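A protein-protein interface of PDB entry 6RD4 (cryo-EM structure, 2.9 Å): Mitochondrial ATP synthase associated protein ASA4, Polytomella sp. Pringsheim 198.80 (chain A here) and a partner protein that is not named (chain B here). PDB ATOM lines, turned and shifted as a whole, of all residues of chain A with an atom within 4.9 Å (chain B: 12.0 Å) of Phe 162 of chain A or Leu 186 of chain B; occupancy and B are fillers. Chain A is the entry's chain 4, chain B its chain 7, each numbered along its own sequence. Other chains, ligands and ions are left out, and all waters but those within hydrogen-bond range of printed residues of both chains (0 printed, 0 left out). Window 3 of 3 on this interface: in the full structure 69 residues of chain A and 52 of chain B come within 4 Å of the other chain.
Of chain B, only Leu 186 (3.2 Å) comes within 4 Å of Phe 162 of chain A. Of chain A, only Val 122 (3.7 Å), Leu 123 (3.8 Å), Leu 138 (3.8 Å), Phe 155 (3.96 Å) and Phe 162 (3.2 Å) come within 4 Å of Leu 186 of chain B. Val 119 of chain A touches none of the printed residues of chain B. Of the printed residues of chain B, Val 122 of chain A touches Leu 186. Leu 138 of chain A touches just these residues of chain B: Phe 182 (3.8 Å) and Leu 186 (3.8 Å). No residue of chain B comes within 4 Å of Val 153 of chain A. Gly 157 of chain A touches none of the printed residues of chain B. Thr 159 of chain A touches none of the printed residues of chain B. Glu 160 of chain A touches none of the printed residues of chain B. Gly 161 of chain A touches none of the printed residues of chain B. No residue of chain B comes within 4 Å of Lys 163 of chain A. Of the printed residues of chain A, Phe 182 of chain B touches Leu 123 and Leu 138. Of the printed residues of chain B, Phe 155 of chain A touches Leu 186 and Gln 190. Of the printed residues of chain A, Gln 190 of chain B touches Phe 155. Val 177 of chain B touches none of the printed residues of chain A. The nearest residue of chain A that does not touch Leu 186 of chain B is Phe 165 of chain A (4.1 Å). The nearest printed residue of chain A that does not touch Gln 190 of chain B is Gly 157 of chain A (4.6 Å).
Of the 14 printed residues of chain B, 4 touch a printed residue of chain A. Printed residues of chain B that touch a printed residue of chain A: Phe 182, Leu 186, Leu 187 and Gln 190. Hydrophobic or aromatic side chains of chain B that line the printed part of chain A: Phe 182, Leu 186 and Leu 187. Among the printed residues, no Asp or Glu carboxylate lies within 4 Å of a Lys or Arg side-chain nitrogen of the other chain.
Among the printed residues, pairs that only touch across the chains: Phe 162 of chain A with Leu 186 of chain B, Phe 155 of chain A with Gln 190 of chain B, Val 122 of chain A with Leu 186 of chain B, Ala 166 of chain A with Leu 187 of chain B, Leu 138 of chain A with Phe 182 of chain B, Leu 138 of chain A with Leu 186 of chain B, Leu 123 of chain A with Leu 186 of chain B, Leu 123 of chain A with Phe 182 of chain B and Phe 155 of chain A with Leu 186 of chain B.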
ATOM      1  N   VAL A 119     -31.563  22.446 -24.446  1.00  0.00           N
ATOM      2  CA  VAL A 119     -31.753  21.183 -23.747  1.00  0.00           C
ATOM      3  C   VAL A 119     -32.429  20.157 -24.647  1.00  0.00           C
ATOM      4  O   VAL A 119     -32.116  18.966 -24.574  1.00  0.00           O
ATOM      5  CB  VAL A 119     -32.531  21.454 -22.450  1.00  0.00           C
ATOM      6  CG1 VAL A 119     -32.924  20.192 -21.753  1.00  0.00           C
ATOM      7  CG2 VAL A 119     -31.675  22.271 -21.527  1.00  0.00           C
ATOM      8  N   VAL A 122     -29.753  18.499 -26.358  1.00  0.00           N
ATOM      9  CA  VAL A 122     -28.986  17.660 -25.443  1.00  0.00           C
ATOM     10  C   VAL A 122     -29.726  16.359 -25.171  1.00  0.00           C
ATOM     11  O   VAL A 122     -29.152  15.271 -25.250  1.00  0.00           O
ATOM     12  CB  VAL A 122     -28.688  18.425 -24.145  1.00  0.00           C
ATOM     13  CG1 VAL A 122     -28.258  17.494 -23.045  1.00  0.00           C
ATOM     14  CG2 VAL A 122     -27.623  19.441 -24.401  1.00  0.00           C
ATOM     15  N   LEU A 123     -31.030  16.445 -24.937  1.00  0.00           N
ATOM     16  CA  LEU A 123     -31.875  15.269 -24.780  1.00  0.00           C
ATOM     17  C   LEU A 123     -32.123  14.523 -26.079  1.00  0.00           C
ATOM     18  O   LEU A 123     -32.923  13.590 -26.073  1.00  0.00           O
ATOM     19  CB  LEU A 123     -33.223  15.661 -24.178  1.00  0.00           C
ATOM     20  CG  LEU A 123     -33.464  15.668 -22.671  1.00  0.00           C
ATOM     21  CD1 LEU A 123     -33.389  14.280 -22.155  1.00  0.00           C
ATOM     22  CD2 LEU A 123     -32.472  16.506 -21.931  1.00  0.00           C
ATOM     23  N   LEU A 138     -37.953  12.894 -19.173  1.00  0.00           N
ATOM     24  CA  LEU A 138     -37.363  14.221 -19.215  1.00  0.00           C
ATOM     25  C   LEU A 138     -37.936  15.053 -20.341  1.00  0.00           C
ATOM     26  O   LEU A 138     -37.969  16.278 -20.232  1.00  0.00           O
ATOM     27  CB  LEU A 138     -35.847  14.135 -19.373  1.00  0.00           C
ATOM     28  CG  LEU A 138     -35.092  13.532 -18.194  1.00  0.00           C
ATOM     29  CD1 LEU A 138     -33.607  13.599 -18.436  1.00  0.00           C
ATOM     30  CD2 LEU A 138     -35.464  14.226 -16.902  1.00  0.00           C
ATOM     31  N   VAL A 153     -35.655  25.887 -23.651  1.00  0.00           N
ATOM     32  CA  VAL A 153     -34.862  25.868 -22.427  1.00  0.00           C
ATOM     33  C   VAL A 153     -33.403  25.713 -22.814  1.00  0.00           C
ATOM     34  O   VAL A 153     -33.042  24.799 -23.562  1.00  0.00           O
ATOM     35  CB  VAL A 153     -35.305  24.750 -21.481  1.00  0.00           C
ATOM     36  CG1 VAL A 153     -34.472  24.790 -20.222  1.00  0.00           C
ATOM     37  CG2 VAL A 153     -36.750  24.903 -21.129  1.00  0.00           C
ATOM     38  N   LEU A 154     -32.569  26.625 -22.340  1.00  0.00           N
ATOM     39  CA  LEU A 154     -31.180  26.675 -22.747  1.00  0.00           C
ATOM     40  C   LEU A 154     -30.322  25.779 -21.870  1.00  0.00           C
ATOM     41  O   LEU A 154     -30.626  25.550 -20.696  1.00  0.00           O
ATOM     42  CB  LEU A 154     -30.655  28.107 -22.693  1.00  0.00           C
ATOM     43  CG  LEU A 154     -31.244  29.077 -23.710  1.00  0.00           C
ATOM     44  CD1 LEU A 154     -30.459  30.369 -23.677  1.00  0.00           C
ATOM     45  CD2 LEU A 154     -31.264  28.482 -25.111  1.00  0.00           C
ATOM     46  N   PHE A 155     -29.240  25.278 -22.459  1.00  0.00           N
ATOM     47  CA  PHE A 155     -28.216  24.543 -21.725  1.00  0.00           C
ATOM     48  C   PHE A 155     -27.176  25.555 -21.241  1.00  0.00           C
ATOM     49  O   PHE A 155     -26.069  25.671 -21.767  1.00  0.00           O
ATOM     50  CB  PHE A 155     -27.616  23.467 -22.621  1.00  0.00           C
ATOM     51  CG  PHE A 155     -27.026  22.311 -21.882  1.00  0.00           C
ATOM     52  CD1 PHE A 155     -27.675  21.763 -20.792  1.00  0.00           C
ATOM     53  CD2 PHE A 155     -25.838  21.742 -22.308  1.00  0.00           C
ATOM     54  CE1 PHE A 155     -27.137  20.694 -20.122  1.00  0.00           C
ATOM     55  CE2 PHE A 155     -25.304  20.663 -21.653  1.00  0.00           C
ATOM     56  CZ  PHE A 155     -25.949  20.149 -20.550  1.00  0.00           C
ATOM     57  N   GLY A 157     -27.469  26.820 -17.444  1.00  0.00           N
ATOM     58  CA  GLY A 157     -27.260  26.639 -16.014  1.00  0.00           C
ATOM     59  C   GLY A 157     -27.536  27.860 -15.182  1.00  0.00           C
ATOM     60  O   GLY A 157     -28.209  27.774 -14.156  1.00  0.00           O
ATOM     61  N   THR A 159     -29.157  30.433 -16.546  1.00  0.00           N
ATOM     62  CA  THR A 159     -30.501  30.806 -16.951  1.00  0.00           C
ATOM     63  C   THR A 159     -31.505  30.260 -15.945  1.00  0.00           C
ATOM     64  O   THR A 159     -31.442  29.089 -15.568  1.00  0.00           O
ATOM     65  CB  THR A 159     -30.788  30.256 -18.343  1.00  0.00           C
ATOM     66  OG1 THR A 159     -29.868  30.832 -19.271  1.00  0.00           O
ATOM     67  CG2 THR A 159     -32.178  30.591 -18.782  1.00  0.00           C
ATOM     68  N   GLU A 160     -32.410  31.119 -15.477  1.00  0.00           N
ATOM     69  CA  GLU A 160     -33.436  30.663 -14.552  1.00  0.00           C
ATOM     70  C   GLU A 160     -34.458  29.775 -15.254  1.00  0.00           C
ATOM     71  O   GLU A 160     -35.092  28.941 -14.600  1.00  0.00           O
ATOM     72  CB  GLU A 160     -34.083  31.885 -13.879  1.00  0.00           C
ATOM     73  CG  GLU A 160     -35.132  31.618 -12.788  1.00  0.00           C
ATOM     74  CD  GLU A 160     -36.541  31.400 -13.315  1.00  0.00           C
ATOM     75  OE1 GLU A 160     -37.389  30.920 -12.537  1.00  0.00           O
ATOM     76  OE2 GLU A 160     -36.807  31.722 -14.490  1.00  0.00           O
ATOM     77  N   GLY A 161     -34.602  29.911 -16.576  1.00  0.00           N
ATOM     78  CA  GLY A 161     -35.451  29.025 -17.356  1.00  0.00           C
ATOM     79  C   GLY A 161     -34.984  27.586 -17.377  1.00  0.00           C
ATOM     80  O   GLY A 161     -35.783  26.686 -17.657  1.00  0.00           O
ATOM     81  N   PHE A 162     -33.704  27.355 -17.099  1.00  0.00           N
ATOM     82  CA  PHE A 162     -33.170  26.028 -16.862  1.00  0.00           C
ATOM     83  C   PHE A 162     -33.279  25.616 -15.404  1.00  0.00           C
ATOM     84  O   PHE A 162     -33.401  24.423 -15.119  1.00  0.00           O
ATOM     85  CB  PHE A 162     -31.706  25.987 -17.308  1.00  0.00           C
ATOM     86  CG  PHE A 162     -31.035  24.661 -17.104  1.00  0.00           C
ATOM     87  CD1 PHE A 162     -31.274  23.611 -17.971  1.00  0.00           C
ATOM     88  CD2 PHE A 162     -30.163  24.465 -16.045  1.00  0.00           C
ATOM     89  CE1 PHE A 162     -30.660  22.398 -17.784  1.00  0.00           C
ATOM     90  CE2 PHE A 162     -29.555  23.258 -15.858  1.00  0.00           C
ATOM     91  CZ  PHE A 162     -29.802  22.228 -16.730  1.00  0.00           C
ATOM     92  N   LYS A 163     -33.259  26.581 -14.480  1.00  0.00           N
ATOM     93  CA  LYS A 163     -33.158  26.270 -13.055  1.00  0.00           C
ATOM     94  C   LYS A 163     -34.415  25.599 -12.520  1.00  0.00           C
ATOM     95  O   LYS A 163     -34.335  24.729 -11.648  1.00  0.00           O
ATOM     96  CB  LYS A 163     -32.883  27.539 -12.258  1.00  0.00           C
ATOM     97  CG  LYS A 163     -31.443  27.939 -12.212  1.00  0.00           C
ATOM     98  CD  LYS A 163     -31.219  28.921 -11.087  1.00  0.00           C
ATOM     99  CE  LYS A 163     -29.828  29.496 -11.160  1.00  0.00           C
ATOM    100  NZ  LYS A 163     -29.616  30.191 -12.457  1.00  0.00           N
ATOM    101  N   LYS A 164     -35.581  26.015 -12.992  1.00  0.00           N
ATOM    102  CA  LYS A 164     -36.822  25.371 -12.598  1.00  0.00           C
ATOM    103  C   LYS A 164     -37.178  24.205 -13.501  1.00  0.00           C
ATOM    104  O   LYS A 164     -38.142  23.489 -13.212  1.00  0.00           O
ATOM    105  CB  LYS A 164     -37.959  26.392 -12.571  1.00  0.00           C
ATOM    106  CG  LYS A 164     -38.234  27.042 -13.904  1.00  0.00           C
ATOM    107  CD  LYS A 164     -39.238  28.164 -13.748  1.00  0.00           C
ATOM    108  CE  LYS A 164     -39.480  28.838 -15.075  1.00  0.00           C
ATOM    109  NZ  LYS A 164     -38.252  29.509 -15.554  1.00  0.00           N
ATOM    110  N   PHE A 165     -36.435  24.009 -14.592  1.00  0.00           N
ATOM    111  CA  PHE A 165     -36.498  22.734 -15.290  1.00  0.00           C
ATOM    112  C   PHE A 165     -35.622  21.702 -14.602  1.00  0.00           C
ATOM    113  O   PHE A 165     -36.039  20.555 -14.421  1.00  0.00           O
ATOM    114  CB  PHE A 165     -36.078  22.909 -16.744  1.00  0.00           C
ATOM    115  CG  PHE A 165     -35.513  21.669 -17.368  1.00  0.00           C
ATOM    116  CD1 PHE A 165     -36.331  20.596 -17.689  1.00  0.00           C
ATOM    117  CD2 PHE A 165     -34.169  21.589 -17.666  1.00  0.00           C
ATOM    118  CE1 PHE A 165     -35.809  19.457 -18.268  1.00  0.00           C
ATOM    119  CE2 PHE A 165     -33.645  20.461 -18.244  1.00  0.00           C
ATOM    120  CZ  PHE A 165     -34.466  19.392 -18.548  1.00  0.00           C
ATOM    121  N   ALA A 166     -34.417  22.103 -14.199  1.00  0.00           N
ATOM    122  CA  ALA A 166     -33.537  21.207 -13.465  1.00  0.00           C
ATOM    123  C   ALA A 166     -34.083  20.878 -12.083  1.00  0.00           C
ATOM    124  O   ALA A 166     -33.760  19.826 -11.528  1.00  0.00           O
ATOM    125  CB  ALA A 166     -32.148  21.822 -13.345  1.00  0.00           C
ATOM    126  N   ALA A 167     -34.899  21.750 -11.505  1.00  0.00           N
ATOM    127  CA  ALA A 167     -35.549  21.409 -10.251  1.00  0.00           C
ATOM    128  C   ALA A 167     -36.703  20.443 -10.456  1.00  0.00           C
ATOM    129  O   ALA A 167     -37.091  19.751  -9.510  1.00  0.00           O
ATOM    130  CB  ALA A 167     -36.046  22.668  -9.547  1.00  0.00           C
ATOM    131  N   VAL B 177     -26.666   2.870 -14.475  1.00  0.00           N
ATOM    132  CA  VAL B 177     -25.502   3.718 -14.266  1.00  0.00           C
ATOM    133  C   VAL B 177     -25.515   4.877 -15.245  1.00  0.00           C
ATOM    134  O   VAL B 177     -25.294   6.026 -14.863  1.00  0.00           O
ATOM    135  CB  VAL B 177     -24.217   2.887 -14.374  1.00  0.00           C
ATOM    136  CG1 VAL B 177     -23.011   3.759 -14.438  1.00  0.00           C
ATOM    137  CG2 VAL B 177     -24.108   1.990 -13.195  1.00  0.00           C
ATOM    138  N   ALA B 178     -25.824   4.612 -16.507  1.00  0.00           N
ATOM    139  CA  ALA B 178     -25.805   5.668 -17.506  1.00  0.00           C
ATOM    140  C   ALA B 178     -26.976   6.627 -17.384  1.00  0.00           C
ATOM    141  O   ALA B 178     -26.929   7.706 -17.972  1.00  0.00           O
ATOM    142  CB  ALA B 178     -25.785   5.072 -18.904  1.00  0.00           C
ATOM    143  N   ASP B 179     -28.026   6.259 -16.655  1.00  0.00           N
ATOM    144  CA  ASP B 179     -29.054   7.230 -16.308  1.00  0.00           C
ATOM    145  C   ASP B 179     -28.646   8.027 -15.091  1.00  0.00           C
ATOM    146  O   ASP B 179     -28.943   9.217 -14.998  1.00  0.00           O
ATOM    147  CB  ASP B 179     -30.380   6.537 -16.040  1.00  0.00           C
ATOM    148  CG  ASP B 179     -30.995   5.973 -17.288  1.00  0.00           C
ATOM    149  OD1 ASP B 179     -30.424   6.172 -18.375  1.00  0.00           O
ATOM    150  OD2 ASP B 179     -32.046   5.310 -17.183  1.00  0.00           O
ATOM    151  N   GLY B 180     -27.961   7.385 -14.152  1.00  0.00           N
ATOM    152  CA  GLY B 180     -27.471   8.089 -12.986  1.00  0.00           C
ATOM    153  C   GLY B 180     -26.363   9.059 -13.306  1.00  0.00           C
ATOM    154  O   GLY B 180     -26.140  10.010 -12.561  1.00  0.00           O
ATOM    155  N   ALA B 181     -25.651   8.834 -14.393  1.00  0.00           N
ATOM    156  CA  ALA B 181     -24.635   9.760 -14.839  1.00  0.00           C
ATOM    157  C   ALA B 181     -25.148  10.741 -15.871  1.00  0.00           C
ATOM    158  O   ALA B 181     -24.376  11.567 -16.350  1.00  0.00           O
ATOM    159  CB  ALA B 181     -23.449   9.004 -15.401  1.00  0.00           C
ATOM    160  N   PHE B 182     -26.412  10.640 -16.255  1.00  0.00           N
ATOM    161  CA  PHE B 182     -27.059  11.726 -16.973  1.00  0.00           C
ATOM    162  C   PHE B 182     -27.622  12.750 -16.014  1.00  0.00           C
ATOM    163  O   PHE B 182     -27.661  13.937 -16.334  1.00  0.00           O
ATOM    164  CB  PHE B 182     -28.175  11.182 -17.845  1.00  0.00           C
ATOM    165  CG  PHE B 182     -28.566  12.075 -18.960  1.00  0.00           C
ATOM    166  CD1 PHE B 182     -27.676  12.378 -19.960  1.00  0.00           C
ATOM    167  CD2 PHE B 182     -29.843  12.571 -19.038  1.00  0.00           C
ATOM    168  CE1 PHE B 182     -28.050  13.178 -21.003  1.00  0.00           C
ATOM    169  CE2 PHE B 182     -30.214  13.373 -20.080  1.00  0.00           C
ATOM    170  CZ  PHE B 182     -29.315  13.672 -21.062  1.00  0.00           C
ATOM    171  N   THR B 183     -28.055  12.302 -14.839  1.00  0.00           N
ATOM    172  CA  THR B 183     -28.488  13.210 -13.788  1.00  0.00           C
ATOM    173  C   THR B 183     -27.344  14.108 -13.329  1.00  0.00           C
ATOM    174  O   THR B 183     -27.542  15.300 -13.090  1.00  0.00           O
ATOM    175  CB  THR B 183     -29.062  12.386 -12.643  1.00  0.00           C
ATOM    176  OG1 THR B 183     -30.302  11.818 -13.064  1.00  0.00           O
ATOM    177  CG2 THR B 183     -29.302  13.206 -11.415  1.00  0.00           C
ATOM    178  N   ASN B 184     -26.129  13.576 -13.256  1.00  0.00           N
ATOM    179  CA  ASN B 184     -24.991  14.438 -12.968  1.00  0.00           C
ATOM    180  C   ASN B 184     -24.670  15.345 -14.145  1.00  0.00           C
ATOM    181  O   ASN B 184     -24.266  16.494 -13.953  1.00  0.00           O
ATOM    182  CB  ASN B 184     -23.774  13.607 -12.606  1.00  0.00           C
ATOM    183  CG  ASN B 184     -22.551  14.450 -12.418  1.00  0.00           C
ATOM    184  OD1 ASN B 184     -21.569  14.318 -13.140  1.00  0.00           O
ATOM    185  ND2 ASN B 184     -22.621  15.359 -11.472  1.00  0.00           N
ATOM    186  N   PHE B 185     -24.856  14.862 -15.364  1.00  0.00           N
ATOM    187  CA  PHE B 185     -24.489  15.665 -16.520  1.00  0.00           C
ATOM    188  C   PHE B 185     -25.518  16.738 -16.803  1.00  0.00           C
ATOM    189  O   PHE B 185     -25.159  17.837 -17.232  1.00  0.00           O
ATOM    190  CB  PHE B 185     -24.328  14.772 -17.738  1.00  0.00           C
ATOM    191  CG  PHE B 185     -24.107  15.515 -19.008  1.00  0.00           C
ATOM    192  CD1 PHE B 185     -25.122  15.645 -19.936  1.00  0.00           C
ATOM    193  CD2 PHE B 185     -22.877  16.054 -19.294  1.00  0.00           C
ATOM    194  CE1 PHE B 185     -24.915  16.314 -21.107  1.00  0.00           C
ATOM    195  CE2 PHE B 185     -22.667  16.719 -20.468  1.00  0.00           C
ATOM    196  CZ  PHE B 185     -23.689  16.848 -21.370  1.00  0.00           C
ATOM    197  N   LEU B 186     -26.793  16.440 -16.591  1.00  0.00           N
ATOM    198  CA  LEU B 186     -27.827  17.396 -16.957  1.00  0.00           C
ATOM    199  C   LEU B 186     -28.041  18.403 -15.841  1.00  0.00           C
ATOM    200  O   LEU B 186     -28.143  19.602 -16.091  1.00  0.00           O
ATOM    201  CB  LEU B 186     -29.124  16.666 -17.278  1.00  0.00           C
ATOM    202  CG  LEU B 186     -30.105  17.415 -18.151  1.00  0.00           C
ATOM    203  CD1 LEU B 186     -29.482  17.559 -19.508  1.00  0.00           C
ATOM    204  CD2 LEU B 186     -31.385  16.652 -18.246  1.00  0.00           C
ATOM    205  N   LEU B 187     -28.067  17.941 -14.595  1.00  0.00           N
ATOM    206  CA  LEU B 187     -28.297  18.821 -13.460  1.00  0.00           C
ATOM    207  C   LEU B 187     -27.015  19.433 -12.923  1.00  0.00           C
ATOM    208  O   LEU B 187     -26.934  19.743 -11.731  1.00  0.00           O
ATOM    209  CB  LEU B 187     -29.028  18.089 -12.340  1.00  0.00           C
ATOM    210  CG  LEU B 187     -30.274  17.263 -12.635  1.00  0.00           C
ATOM    211  CD1 LEU B 187     -30.930  16.953 -11.323  1.00  0.00           C
ATOM    212  CD2 LEU B 187     -31.234  17.956 -13.563  1.00  0.00           C
ATOM    213  N   SER B 188     -25.999  19.572 -13.754  1.00  0.00           N
ATOM    214  CA  SER B 188     -24.932  20.526 -13.531  1.00  0.00           C
ATOM    215  C   SER B 188     -24.985  21.560 -14.644  1.00  0.00           C
ATOM    216  O   SER B 188     -25.751  21.435 -15.601  1.00  0.00           O
ATOM    217  CB  SER B 188     -23.574  19.834 -13.467  1.00  0.00           C
ATOM    218  OG  SER B 188     -23.605  18.770 -12.541  1.00  0.00           O
ATOM    219  N   LYS B 189     -24.174  22.599 -14.506  1.00  0.00           N
ATOM    220  CA  LYS B 189     -24.178  23.681 -15.479  1.00  0.00           C
ATOM    221  C   LYS B 189     -23.532  23.214 -16.779  1.00  0.00           C
ATOM    222  O   LYS B 189     -22.403  22.711 -16.776  1.00  0.00           O
ATOM    223  CB  LYS B 189     -23.499  24.918 -14.887  1.00  0.00           C
ATOM    224  CG  LYS B 189     -22.081  24.722 -14.373  1.00  0.00           C
ATOM    225  CD  LYS B 189     -21.613  25.903 -13.590  1.00  0.00           C
ATOM    226  CE  LYS B 189     -22.370  25.931 -12.289  1.00  0.00           C
ATOM    227  NZ  LYS B 189     -22.097  24.707 -11.499  1.00  0.00           N
ATOM    228  N   GLN B 190     -24.303  23.330 -17.863  1.00  0.00           N
ATOM    229  CA  GLN B 190     -24.005  22.978 -19.262  1.00  0.00           C
ATOM    230  C   GLN B 190     -22.953  21.905 -19.546  1.00  0.00           C
ATOM    231  O   GLN B 190     -22.969  20.831 -18.945  1.00  0.00           O
ATOM    232  CB  GLN B 190     -23.613  24.230 -20.045  1.00  0.00           C
ATOM    233  CG  GLN B 190     -22.204  24.763 -19.811  1.00  0.00           C
ATOM    234  CD  GLN B 190     -22.123  25.874 -18.778  1.00  0.00           C
ATOM    235  OE1 GLN B 190     -23.009  26.045 -17.950  1.00  0.00           O
ATOM    236  NE2 GLN B 190     -21.054  26.655 -18.848  1.00  0.00           N
